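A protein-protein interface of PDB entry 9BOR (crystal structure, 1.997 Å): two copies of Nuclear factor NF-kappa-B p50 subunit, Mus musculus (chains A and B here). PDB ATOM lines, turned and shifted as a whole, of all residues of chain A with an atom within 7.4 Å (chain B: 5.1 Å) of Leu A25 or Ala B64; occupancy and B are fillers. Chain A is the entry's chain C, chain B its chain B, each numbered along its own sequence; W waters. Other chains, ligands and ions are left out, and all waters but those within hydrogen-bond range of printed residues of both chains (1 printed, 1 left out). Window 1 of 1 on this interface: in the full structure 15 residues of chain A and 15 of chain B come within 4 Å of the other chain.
The backbone NH (N) of Val A7 lies within hydrogen-bond range of the backbone carbonyl oxygen (O) of Leu A25, 2.7 Å away. OD1 of Asp A10 lies within hydrogen-bond range of N of Tyr A23. The backbone carbonyl oxygen (O) of Arg A8 lies within hydrogen-bond range of the backbone NH (N) of Leu A25, at 2.7 Å. The backbone NH (N) of Cys B26 lies within hydrogen-bond range of the backbone carbonyl oxygen (O) of Phe B63, at 3.0 Å. O of Asp B58 lies within hydrogen-bond range of N of Val B66 (3.1 Å). The backbone carbonyl oxygen (O) of Phe A63 sits at hydrogen-bond distance from the backbone NH (N) of Cys A26 (3.0 Å).
Among the printed residues, merely in contact across the chains: Val A7 with His B60, Arg A8 with Tyr B23, Arg A8 with Val B66, Tyr A23 with Tyr B23, Tyr A23 with Leu B25, Leu A25 with Tyr B23, Leu A25 with His B60, Leu A25 with Ala B64, Leu A25 with Val B66, His A60 with Leu B25, Phe A63 with Phe B63 and Ala A64 with Leu B25.
The guanidinium group of Arg A8 is in salt-bridge range of the side-chain carboxylate of Asp B58 (3.3 Å). NE2 of His B60 lies within hydrogen-bond range of O of Cys A26. The backbone carbonyl oxygen (O) of Phe B63 sits at hydrogen-bond distance from a ring nitrogen (NE2) of His A60, at 2.9 Å. OH of Tyr B23 lies within hydrogen-bond range of N of Asp A10. The backbone carbonyl oxygen (O) of Cys B26 sits at hydrogen-bond distance from a ring nitrogen (NE2) of His A60 (2.9 Å). OH of Tyr B23 sits at hydrogen-bond distance from O of Met A9. A ring nitrogen (NE2) of His B60 is in hydrogen-bond range of the backbone carbonyl oxygen (O) of Phe A63.
Of the printed residues of chain B, Leu A25 touches Tyr B23, His B60, Ala B64 and Val B66. Of the printed residues of chain B, Phe A63 touches His B60 and Phe B63. Leu B24 touches none of the printed residues of chain A. Of the printed residues of chain A, Asp B58 touches Arg A8. The nearest printed residue of chain A that does not touch Ala B64 is His A60 (5.1 Å).
Tyr A23 touches its own counterpart, Tyr B23. Leu A25 touches His B60, and with the chains exchanged His A60 touches Leu B25. Leu A25 touches Ala B64, and with the chains exchanged Ala A64 touches Leu B25. His A60 touches Phe B63, and with the chains exchanged Phe A63 touches His B60. Of the 19 pairs that touch across the chains among the printed residues, 12 have their exchanged pair printed and touching as well.
Water W1 bridges O of Asp B58 and NH1 of Arg A8.
Of the 18 printed residues of chain A, 10 touch a printed residue of chain B. Printed residues of chain A that touch a printed residue of chain B: Val A7, Arg A8, Met A9, Asp A10, Tyr A23, Leu A25, Cys A26, His A60, Phe A63 and Ala A64. Hydrophobic or aromatic side chains of chain A that line the printed part of chain B: Val A7, Tyr A23, Leu A25, His A60, Phe A63 and Ala A64. Along chain A the printed residues that touch a printed residue of chain B span positions 7 to 64.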
ATOM      1  N   LYS A   5      -3.562 -12.071  22.322  1.00  0.00           N
ATOM      2  CA  LYS A   5      -4.380 -11.198  21.499  1.00  0.00           C
ATOM      3  C   LYS A   5      -3.657  -9.909  21.124  1.00  0.00           C
ATOM      4  O   LYS A   5      -3.092  -9.225  21.979  1.00  0.00           O
ATOM      5  CB  LYS A   5      -5.689 -10.867  22.221  1.00  0.00           C
ATOM      6  CG  LYS A   5      -6.646 -10.008  21.411  1.00  0.00           C
ATOM      7  CD  LYS A   5      -7.887  -9.668  22.219  1.00  0.00           C
ATOM      8  CE  LYS A   5      -8.789 -10.880  22.433  1.00  0.00           C
ATOM      9  NZ  LYS A   5      -9.508 -11.266  21.183  1.00  0.00           N
ATOM     10  N   ILE A   6      -3.673  -9.597  19.833  1.00  0.00           N
ATOM     11  CA  ILE A   6      -3.248  -8.291  19.356  1.00  0.00           C
ATOM     12  C   ILE A   6      -4.449  -7.358  19.371  1.00  0.00           C
ATOM     13  O   ILE A   6      -5.438  -7.607  18.688  1.00  0.00           O
ATOM     14  CB  ILE A   6      -2.665  -8.359  17.941  1.00  0.00           C
ATOM     15  CG1 ILE A   6      -1.454  -9.292  17.904  1.00  0.00           C
ATOM     16  CG2 ILE A   6      -2.311  -6.952  17.452  1.00  0.00           C
ATOM     17  CD1 ILE A   6      -0.882  -9.502  16.488  1.00  0.00           C
ATOM     18  N   VAL A   7      -4.366  -6.284  20.146  1.00  0.00           N
ATOM     19  CA  VAL A   7      -5.502  -5.394  20.336  1.00  0.00           C
ATOM     20  C   VAL A   7      -5.439  -4.219  19.361  1.00  0.00           C
ATOM     21  O   VAL A   7      -6.465  -3.664  18.974  1.00  0.00           O
ATOM     22  CB  VAL A   7      -5.563  -4.882  21.792  1.00  0.00           C
ATOM     23  CG1 VAL A   7      -6.729  -3.927  21.988  1.00  0.00           C
ATOM     24  CG2 VAL A   7      -5.696  -6.061  22.746  1.00  0.00           C
ATOM     25  N   ARG A   8      -4.230  -3.858  18.951  1.00  0.00           N
ATOM     26  CA  ARG A   8      -4.047  -2.715  18.064  1.00  0.00           C
ATOM     27  C   ARG A   8      -2.617  -2.680  17.551  1.00  0.00           C
ATOM     28  O   ARG A   8      -1.698  -3.058  18.275  1.00  0.00           O
ATOM     29  CB  ARG A   8      -4.370  -1.413  18.801  1.00  0.00           C
ATOM     30  CG  ARG A   8      -5.152  -0.409  17.989  1.00  0.00           C
ATOM     31  CD  ARG A   8      -5.505   0.818  18.817  1.00  0.00           C
ATOM     32  NE  ARG A   8      -6.089   1.867  17.985  1.00  0.00           N
ATOM     33  CZ  ARG A   8      -6.961   2.769  18.425  1.00  0.00           C
ATOM     34  NH1 ARG A   8      -7.353   2.755  19.693  1.00  0.00           N
ATOM     35  NH2 ARG A   8      -7.442   3.682  17.595  1.00  0.00           N
ATOM     36  N   MET A   9      -2.437  -2.225  16.312  1.00  0.00           N
ATOM     37  CA  MET A   9      -1.109  -2.025  15.731  1.00  0.00           C
ATOM     38  C   MET A   9      -1.062  -0.683  15.013  1.00  0.00           C
ATOM     39  O   MET A   9      -1.973  -0.364  14.249  1.00  0.00           O
ATOM     40  CB  MET A   9      -0.759  -3.132  14.736  1.00  0.00           C
ATOM     41  CG  MET A   9      -0.638  -4.503  15.312  1.00  0.00           C
ATOM     42  SD  MET A   9      -0.324  -5.693  13.999  1.00  0.00           S
ATOM     43  CE  MET A   9       1.293  -5.176  13.419  1.00  0.00           C
ATOM     44  N   ASP A  10      -0.010   0.099  15.230  1.00  0.00           N
ATOM     45  CA  ASP A  10       0.043   1.426  14.607  1.00  0.00           C
ATOM     46  C   ASP A  10       0.417   1.357  13.122  1.00  0.00           C
ATOM     47  O   ASP A  10       0.327   2.355  12.412  1.00  0.00           O
ATOM     48  CB  ASP A  10       1.013   2.352  15.358  1.00  0.00           C
ATOM     49  CG  ASP A  10       2.480   1.970  15.183  1.00  0.00           C
ATOM     50  OD1 ASP A  10       2.795   0.856  14.714  1.00  0.00           O
ATOM     51  OD2 ASP A  10       3.333   2.802  15.548  1.00  0.00           O
ATOM     52  N   ILE A  22       7.372  -0.725  14.614  1.00  0.00           N
ATOM     53  CA  ILE A  22       5.935  -0.865  14.822  1.00  0.00           C
ATOM     54  C   ILE A  22       5.600  -0.928  16.314  1.00  0.00           C
ATOM     55  O   ILE A  22       6.313  -1.571  17.090  1.00  0.00           O
ATOM     56  CB  ILE A  22       5.390  -2.131  14.124  1.00  0.00           C
ATOM     57  CG1 ILE A  22       5.573  -2.028  12.610  1.00  0.00           C
ATOM     58  CG2 ILE A  22       3.917  -2.369  14.468  1.00  0.00           C
ATOM     59  CD1 ILE A  22       4.929  -3.164  11.859  1.00  0.00           C
ATOM     60  N   TYR A  23       4.533  -0.234  16.705  1.00  0.00           N
ATOM     61  CA  TYR A  23       3.970  -0.325  18.049  1.00  0.00           C
ATOM     62  C   TYR A  23       2.758  -1.242  18.019  1.00  0.00           C
ATOM     63  O   TYR A  23       1.827  -1.020  17.245  1.00  0.00           O
ATOM     64  CB  TYR A  23       3.548   1.048  18.586  1.00  0.00           C
ATOM     65  CG  TYR A  23       4.652   1.964  19.077  1.00  0.00           C
ATOM     66  CD1 TYR A  23       5.825   2.148  18.341  1.00  0.00           C
ATOM     67  CD2 TYR A  23       4.491   2.698  20.253  1.00  0.00           C
ATOM     68  CE1 TYR A  23       6.826   3.017  18.786  1.00  0.00           C
ATOM     69  CE2 TYR A  23       5.478   3.565  20.705  1.00  0.00           C
ATOM     70  CZ  TYR A  23       6.643   3.725  19.962  1.00  0.00           C
ATOM     71  OH  TYR A  23       7.621   4.587  20.405  1.00  0.00           O
ATOM     72  N   LEU A  24       2.771  -2.257  18.878  1.00  0.00           N
ATOM     73  CA  LEU A  24       1.692  -3.230  18.953  1.00  0.00           C
ATOM     74  C   LEU A  24       1.115  -3.240  20.369  1.00  0.00           C
ATOM     75  O   LEU A  24       1.861  -3.305  21.337  1.00  0.00           O
ATOM     76  CB  LEU A  24       2.218  -4.615  18.555  1.00  0.00           C
ATOM     77  CG  LEU A  24       1.330  -5.860  18.569  1.00  0.00           C
ATOM     78  CD1 LEU A  24       1.806  -6.854  17.510  1.00  0.00           C
ATOM     79  CD2 LEU A  24       1.322  -6.518  19.953  1.00  0.00           C
ATOM     80  N   LEU A  25      -0.205  -3.146  20.493  1.00  0.00           N
ATOM     81  CA  LEU A  25      -0.839  -3.229  21.810  1.00  0.00           C
ATOM     82  C   LEU A  25      -1.438  -4.614  21.954  1.00  0.00           C
ATOM     83  O   LEU A  25      -2.057  -5.124  21.022  1.00  0.00           O
ATOM     84  CB  LEU A  25      -1.917  -2.146  21.991  1.00  0.00           C
ATOM     85  CG  LEU A  25      -1.497  -0.711  21.655  1.00  0.00           C
ATOM     86  CD1 LEU A  25      -2.617   0.278  21.994  1.00  0.00           C
ATOM     87  CD2 LEU A  25      -0.213  -0.351  22.391  1.00  0.00           C
ATOM     88  N   CYS A  26      -1.255  -5.228  23.115  1.00  0.00           N
ATOM     89  CA  CYS A  26      -1.652  -6.619  23.272  1.00  0.00           C
ATOM     90  C   CYS A  26      -2.298  -6.902  24.620  1.00  0.00           C
ATOM     91  O   CYS A  26      -2.208  -6.097  25.552  1.00  0.00           O
ATOM     92  CB  CYS A  26      -0.432  -7.528  23.065  1.00  0.00           C
ATOM     93  SG  CYS A  26       0.981  -7.169  24.156  1.00  0.00           S
ATOM     94  N   ASP A  27      -2.972  -8.044  24.720  1.00  0.00           N
ATOM     95  CA  ASP A  27      -3.334  -8.573  26.026  1.00  0.00           C
ATOM     96  C   ASP A  27      -2.040  -8.919  26.753  1.00  0.00           C
ATOM     97  O   ASP A  27      -0.974  -8.988  26.132  1.00  0.00           O
ATOM     98  CB  ASP A  27      -4.233  -9.806  25.910  1.00  0.00           C
ATOM     99  CG  ASP A  27      -5.702  -9.450  25.829  1.00  0.00           C
ATOM    100  OD1 ASP A  27      -6.075  -8.356  26.299  1.00  0.00           O
ATOM    101  OD2 ASP A  27      -6.487 -10.271  25.305  1.00  0.00           O
ATOM    102  N   HIS A  60       6.551  -3.297  26.792  1.00  0.00           N
ATOM    103  CA  HIS A  60       6.221  -2.208  27.700  1.00  0.00           C
ATOM    104  C   HIS A  60       5.162  -2.623  28.696  1.00  0.00           C
ATOM    105  O   HIS A  60       3.983  -2.717  28.344  1.00  0.00           O
ATOM    106  CB  HIS A  60       5.743  -0.976  26.915  1.00  0.00           C
ATOM    107  CG  HIS A  60       5.202   0.118  27.786  1.00  0.00           C
ATOM    108  ND1 HIS A  60       5.990   0.825  28.667  1.00  0.00           N
ATOM    109  CD2 HIS A  60       3.947   0.605  27.928  1.00  0.00           C
ATOM    110  CE1 HIS A  60       5.244   1.710  29.307  1.00  0.00           C
ATOM    111  NE2 HIS A  60       4.003   1.599  28.874  1.00  0.00           N
ATOM    112  N   PHE A  63       2.018  -5.000  28.197  1.00  0.00           N
ATOM    113  CA  PHE A  63       0.810  -4.706  27.414  1.00  0.00           C
ATOM    114  C   PHE A  63       1.066  -4.077  26.049  1.00  0.00           C
ATOM    115  O   PHE A  63       0.123  -3.773  25.310  1.00  0.00           O
ATOM    116  CB  PHE A  63      -0.120  -3.795  28.215  1.00  0.00           C
ATOM    117  CG  PHE A  63      -0.910  -4.521  29.262  1.00  0.00           C
ATOM    118  CD1 PHE A  63      -1.902  -5.421  28.893  1.00  0.00           C
ATOM    119  CD2 PHE A  63      -0.671  -4.306  30.610  1.00  0.00           C
ATOM    120  CE1 PHE A  63      -2.642  -6.090  29.852  1.00  0.00           C
ATOM    121  CE2 PHE A  63      -1.405  -4.975  31.570  1.00  0.00           C
ATOM    122  CZ  PHE A  63      -2.392  -5.868  31.190  1.00  0.00           C
ATOM    123  N   ALA A  64       2.335  -3.897  25.708  1.00  0.00           N
ATOM    124  CA  ALA A  64       2.694  -3.319  24.418  1.00  0.00           C
ATOM    125  C   ALA A  64       4.076  -3.787  24.021  1.00  0.00           C
ATOM    126  O   ALA A  64       4.904  -4.089  24.886  1.00  0.00           O
ATOM    127  CB  ALA A  64       2.640  -1.795  24.472  1.00  0.00           C
ATOM    128  N   ILE A  65       4.313  -3.869  22.714  1.00  0.00           N
ATOM    129  CA  ILE A  65       5.619  -4.251  22.196  1.00  0.00           C
ATOM    130  C   ILE A  65       6.034  -3.314  21.074  1.00  0.00           C
ATOM    131  O   ILE A  65       5.280  -3.109  20.121  1.00  0.00           O
ATOM    132  CB  ILE A  65       5.636  -5.688  21.653  1.00  0.00           C
ATOM    133  CG1 ILE A  65       5.096  -6.677  22.692  1.00  0.00           C
ATOM    134  CG2 ILE A  65       7.053  -6.070  21.187  1.00  0.00           C
ATOM    135  CD1 ILE A  65       4.930  -8.077  22.157  1.00  0.00           C
ATOM    136  N   PHE A  67       8.671  -3.087  18.122  1.00  0.00           N
ATOM    137  CA  PHE A  67       9.563  -3.995  17.407  1.00  0.00           C
ATOM    138  C   PHE A  67       9.831  -3.508  15.987  1.00  0.00           C
ATOM    139  O   PHE A  67       9.127  -2.630  15.481  1.00  0.00           O
ATOM    140  CB  PHE A  67       8.961  -5.402  17.370  1.00  0.00           C
ATOM    141  CG  PHE A  67       7.726  -5.500  16.520  1.00  0.00           C
ATOM    142  CD1 PHE A  67       6.493  -5.091  17.012  1.00  0.00           C
ATOM    143  CD2 PHE A  67       7.801  -5.981  15.222  1.00  0.00           C
ATOM    144  CE1 PHE A  67       5.359  -5.175  16.225  1.00  0.00           C
ATOM    145  CE2 PHE A  67       6.670  -6.057  14.424  1.00  0.00           C
ATOM    146  CZ  PHE A  67       5.451  -5.654  14.925  1.00  0.00           C
ATOM    147  N   LEU A  87       1.120 -13.032  17.511  1.00  0.00           N
ATOM    148  CA  LEU A  87       1.904 -13.272  18.705  1.00  0.00           C
ATOM    149  C   LEU A  87       2.067 -14.772  18.866  1.00  0.00           C
ATOM    150  O   LEU A  87       1.165 -15.538  18.532  1.00  0.00           O
ATOM    151  CB  LEU A  87       1.219 -12.685  19.939  1.00  0.00           C
ATOM    152  CG  LEU A  87       1.018 -11.176  19.971  1.00  0.00           C
ATOM    153  CD1 LEU A  87       0.001 -10.812  21.046  1.00  0.00           C
ATOM    154  CD2 LEU A  87       2.351 -10.493  20.233  1.00  0.00           C
ATOM    155  N   TYR B  23       0.658   6.641  18.867  1.00  0.00           N
ATOM    156  CA  TYR B  23       0.686   5.681  19.973  1.00  0.00           C
ATOM    157  C   TYR B  23       1.693   6.159  21.002  1.00  0.00           C
ATOM    158  O   TYR B  23       2.871   6.325  20.696  1.00  0.00           O
ATOM    159  CB  TYR B  23       1.071   4.276  19.506  1.00  0.00           C
ATOM    160  CG  TYR B  23       0.003   3.496  18.768  1.00  0.00           C
ATOM    161  CD1 TYR B  23      -0.806   4.101  17.811  1.00  0.00           C
ATOM    162  CD2 TYR B  23      -0.159   2.131  18.996  1.00  0.00           C
ATOM    163  CE1 TYR B  23      -1.764   3.375  17.127  1.00  0.00           C
ATOM    164  CE2 TYR B  23      -1.115   1.396  18.313  1.00  0.00           C
ATOM    165  CZ  TYR B  23      -1.910   2.022  17.382  1.00  0.00           C
ATOM    166  OH  TYR B  23      -2.857   1.296  16.701  1.00  0.00           O
ATOM    167  N   LEU B  24       1.229   6.391  22.220  1.00  0.00           N
ATOM    168  CA  LEU B  24       2.109   6.843  23.287  1.00  0.00           C
ATOM    169  C   LEU B  24       2.175   5.785  24.383  1.00  0.00           C
ATOM    170  O   LEU B  24       1.139   5.339  24.875  1.00  0.00           O
ATOM    171  CB  LEU B  24       1.609   8.182  23.838  1.00  0.00           C
ATOM    172  CG  LEU B  24       2.349   8.891  24.973  1.00  0.00           C
ATOM    173  CD1 LEU B  24       2.129  10.392  24.874  1.00  0.00           C
ATOM    174  CD2 LEU B  24       1.861   8.393  26.312  1.00  0.00           C
ATOM    175  N   LEU B  25       3.382   5.382  24.771  1.00  0.00           N
ATOM    176  CA  LEU B  25       3.525   4.445  25.887  1.00  0.00           C
ATOM    177  C   LEU B  25       3.877   5.216  27.149  1.00  0.00           C
ATOM    178  O   LEU B  25       4.759   6.081  27.141  1.00  0.00           O
ATOM    179  CB  LEU B  25       4.587   3.383  25.587  1.00  0.00           C
ATOM    180  CG  LEU B  25       4.365   2.629  24.275  1.00  0.00           C
ATOM    181  CD1 LEU B  25       5.418   1.539  24.075  1.00  0.00           C
ATOM    182  CD2 LEU B  25       2.955   2.041  24.243  1.00  0.00           C
ATOM    183  N   CYS B  26       3.176   4.915  28.235  1.00  0.00           N
ATOM    184  CA  CYS B  26       3.339   5.681  29.462  1.00  0.00           C
ATOM    185  C   CYS B  26       3.426   4.784  30.676  1.00  0.00           C
ATOM    186  O   CYS B  26       2.989   3.633  30.636  1.00  0.00           O
ATOM    187  CB  CYS B  26       2.172   6.662  29.631  1.00  0.00           C
ATOM    188  SG  CYS B  26       0.519   5.886  29.535  1.00  0.00           S
ATOM    189  N   ASP B  58      -9.518   4.510  24.392  1.00  0.00           N
ATOM    190  CA  ASP B  58      -8.278   4.525  23.624  1.00  0.00           C
ATOM    191  C   ASP B  58      -7.071   4.399  24.540  1.00  0.00           C
ATOM    192  O   ASP B  58      -5.927   4.332  24.078  1.00  0.00           O
ATOM    193  CB  ASP B  58      -8.168   5.804  22.795  1.00  0.00           C
ATOM    194  CG  ASP B  58      -9.214   5.875  21.698  1.00  0.00           C
ATOM    195  OD1 ASP B  58      -9.501   4.818  21.095  1.00  0.00           O
ATOM    196  OD2 ASP B  58      -9.750   6.980  21.450  1.00  0.00           O
ATOM    197  N   VAL B  59      -7.332   4.402  25.843  1.00  0.00           N
ATOM    198  CA  VAL B  59      -6.285   4.175  26.820  1.00  0.00           C
ATOM    199  C   VAL B  59      -6.201   2.673  27.045  1.00  0.00           C
ATOM    200  O   VAL B  59      -7.142   2.052  27.537  1.00  0.00           O
ATOM    201  CB  VAL B  59      -6.547   4.925  28.140  1.00  0.00           C
ATOM    202  CG1 VAL B  59      -5.444   4.642  29.143  1.00  0.00           C
ATOM    203  CG2 VAL B  59      -6.655   6.441  27.872  1.00  0.00           C
ATOM    204  N   HIS B  60      -5.075   2.095  26.650  1.00  0.00           N
ATOM    205  CA  HIS B  60      -4.901   0.650  26.659  1.00  0.00           C
ATOM    206  C   HIS B  60      -4.314   0.170  27.980  1.00  0.00           C
ATOM    207  O   HIS B  60      -3.127   0.354  28.245  1.00  0.00           O
ATOM    208  CB  HIS B  60      -4.007   0.218  25.494  1.00  0.00           C
ATOM    209  CG  HIS B  60      -3.727  -1.250  25.461  1.00  0.00           C
ATOM    210  ND1 HIS B  60      -4.704  -2.191  25.217  1.00  0.00           N
ATOM    211  CD2 HIS B  60      -2.579  -1.943  25.653  1.00  0.00           C
ATOM    212  CE1 HIS B  60      -4.171  -3.399  25.259  1.00  0.00           C
ATOM    213  NE2 HIS B  60      -2.883  -3.276  25.527  1.00  0.00           N
ATOM    214  N   GLN B  62      -4.160   1.092  30.957  1.00  0.00           N
ATOM    215  CA  GLN B  62      -3.460   2.070  31.795  1.00  0.00           C
ATOM    216  C   GLN B  62      -1.998   2.334  31.392  1.00  0.00           C
ATOM    217  O   GLN B  62      -1.320   3.119  32.053  1.00  0.00           O
ATOM    218  CB  GLN B  62      -3.510   1.639  33.271  1.00  0.00           C
ATOM    219  CG  GLN B  62      -4.925   1.441  33.797  1.00  0.00           C
ATOM    220  CD  GLN B  62      -4.978   1.290  35.304  1.00  0.00           C
ATOM    221  OE1 GLN B  62      -4.938   0.178  35.822  1.00  0.00           O
ATOM    222  NE2 GLN B  62      -5.075   2.410  36.016  1.00  0.00           N
ATOM    223  N   PHE B  63      -1.515   1.720  30.310  1.00  0.00           N
ATOM    224  CA  PHE B  63      -0.096   1.849  29.969  1.00  0.00           C
ATOM    225  C   PHE B  63       0.195   2.378  28.568  1.00  0.00           C
ATOM    226  O   PHE B  63       1.358   2.484  28.165  1.00  0.00           O
ATOM    227  CB  PHE B  63       0.603   0.500  30.133  1.00  0.00           C
ATOM    228  CG  PHE B  63       0.813   0.105  31.560  1.00  0.00           C
ATOM    229  CD1 PHE B  63       1.678   0.827  32.367  1.00  0.00           C
ATOM    230  CD2 PHE B  63       0.146  -0.985  32.097  1.00  0.00           C
ATOM    231  CE1 PHE B  63       1.874   0.462  33.693  1.00  0.00           C
ATOM    232  CE2 PHE B  63       0.343  -1.352  33.420  1.00  0.00           C
ATOM    233  CZ  PHE B  63       1.206  -0.626  34.214  1.00  0.00           C
ATOM    234  N   ALA B  64      -0.850   2.681  27.811  1.00  0.00           N
ATOM    235  CA  ALA B  64      -0.658   3.286  26.498  1.00  0.00           C
ATOM    236  C   ALA B  64      -1.873   4.108  26.137  1.00  0.00           C
ATOM    237  O   ALA B  64      -2.978   3.845  26.611  1.00  0.00           O
ATOM    238  CB  ALA B  64      -0.399   2.219  25.435  1.00  0.00           C
ATOM    239  N   ILE B  65      -1.658   5.122  25.315  1.00  0.00           N
ATOM    240  CA  ILE B  65      -2.738   5.966  24.836  1.00  0.00           C
ATOM    241  C   ILE B  65      -2.605   6.131  23.337  1.00  0.00           C
ATOM    242  O   ILE B  65      -1.541   6.496  22.840  1.00  0.00           O
ATOM    243  CB  ILE B  65      -2.734   7.362  25.499  1.00  0.00           C
ATOM    244  CG1 ILE B  65      -2.718   7.238  27.026  1.00  0.00           C
ATOM    245  CG2 ILE B  65      -3.934   8.178  25.023  1.00  0.00           C
ATOM    246  CD1 ILE B  65      -2.531   8.558  27.754  1.00  0.00           C
ATOM    247  N   VAL B  66      -3.681   5.845  22.618  1.00  0.00           N
ATOM    248  CA  VAL B  66      -3.740   6.159  21.202  1.00  0.00           C
ATOM    249  C   VAL B  66      -4.581   7.416  21.035  1.00  0.00           C
ATOM    250  O   VAL B  66      -5.710   7.477  21.521  1.00  0.00           O
ATOM    251  CB  VAL B  66      -4.336   5.000  20.388  1.00  0.00           C
ATOM    252  CG1 VAL B  66      -4.427   5.390  18.926  1.00  0.00           C
ATOM    253  CG2 VAL B  66      -3.486   3.745  20.569  1.00  0.00           C
HETATM  254  O   HOH W   1      -5.957   1.981  22.406  1.00  0.00           O
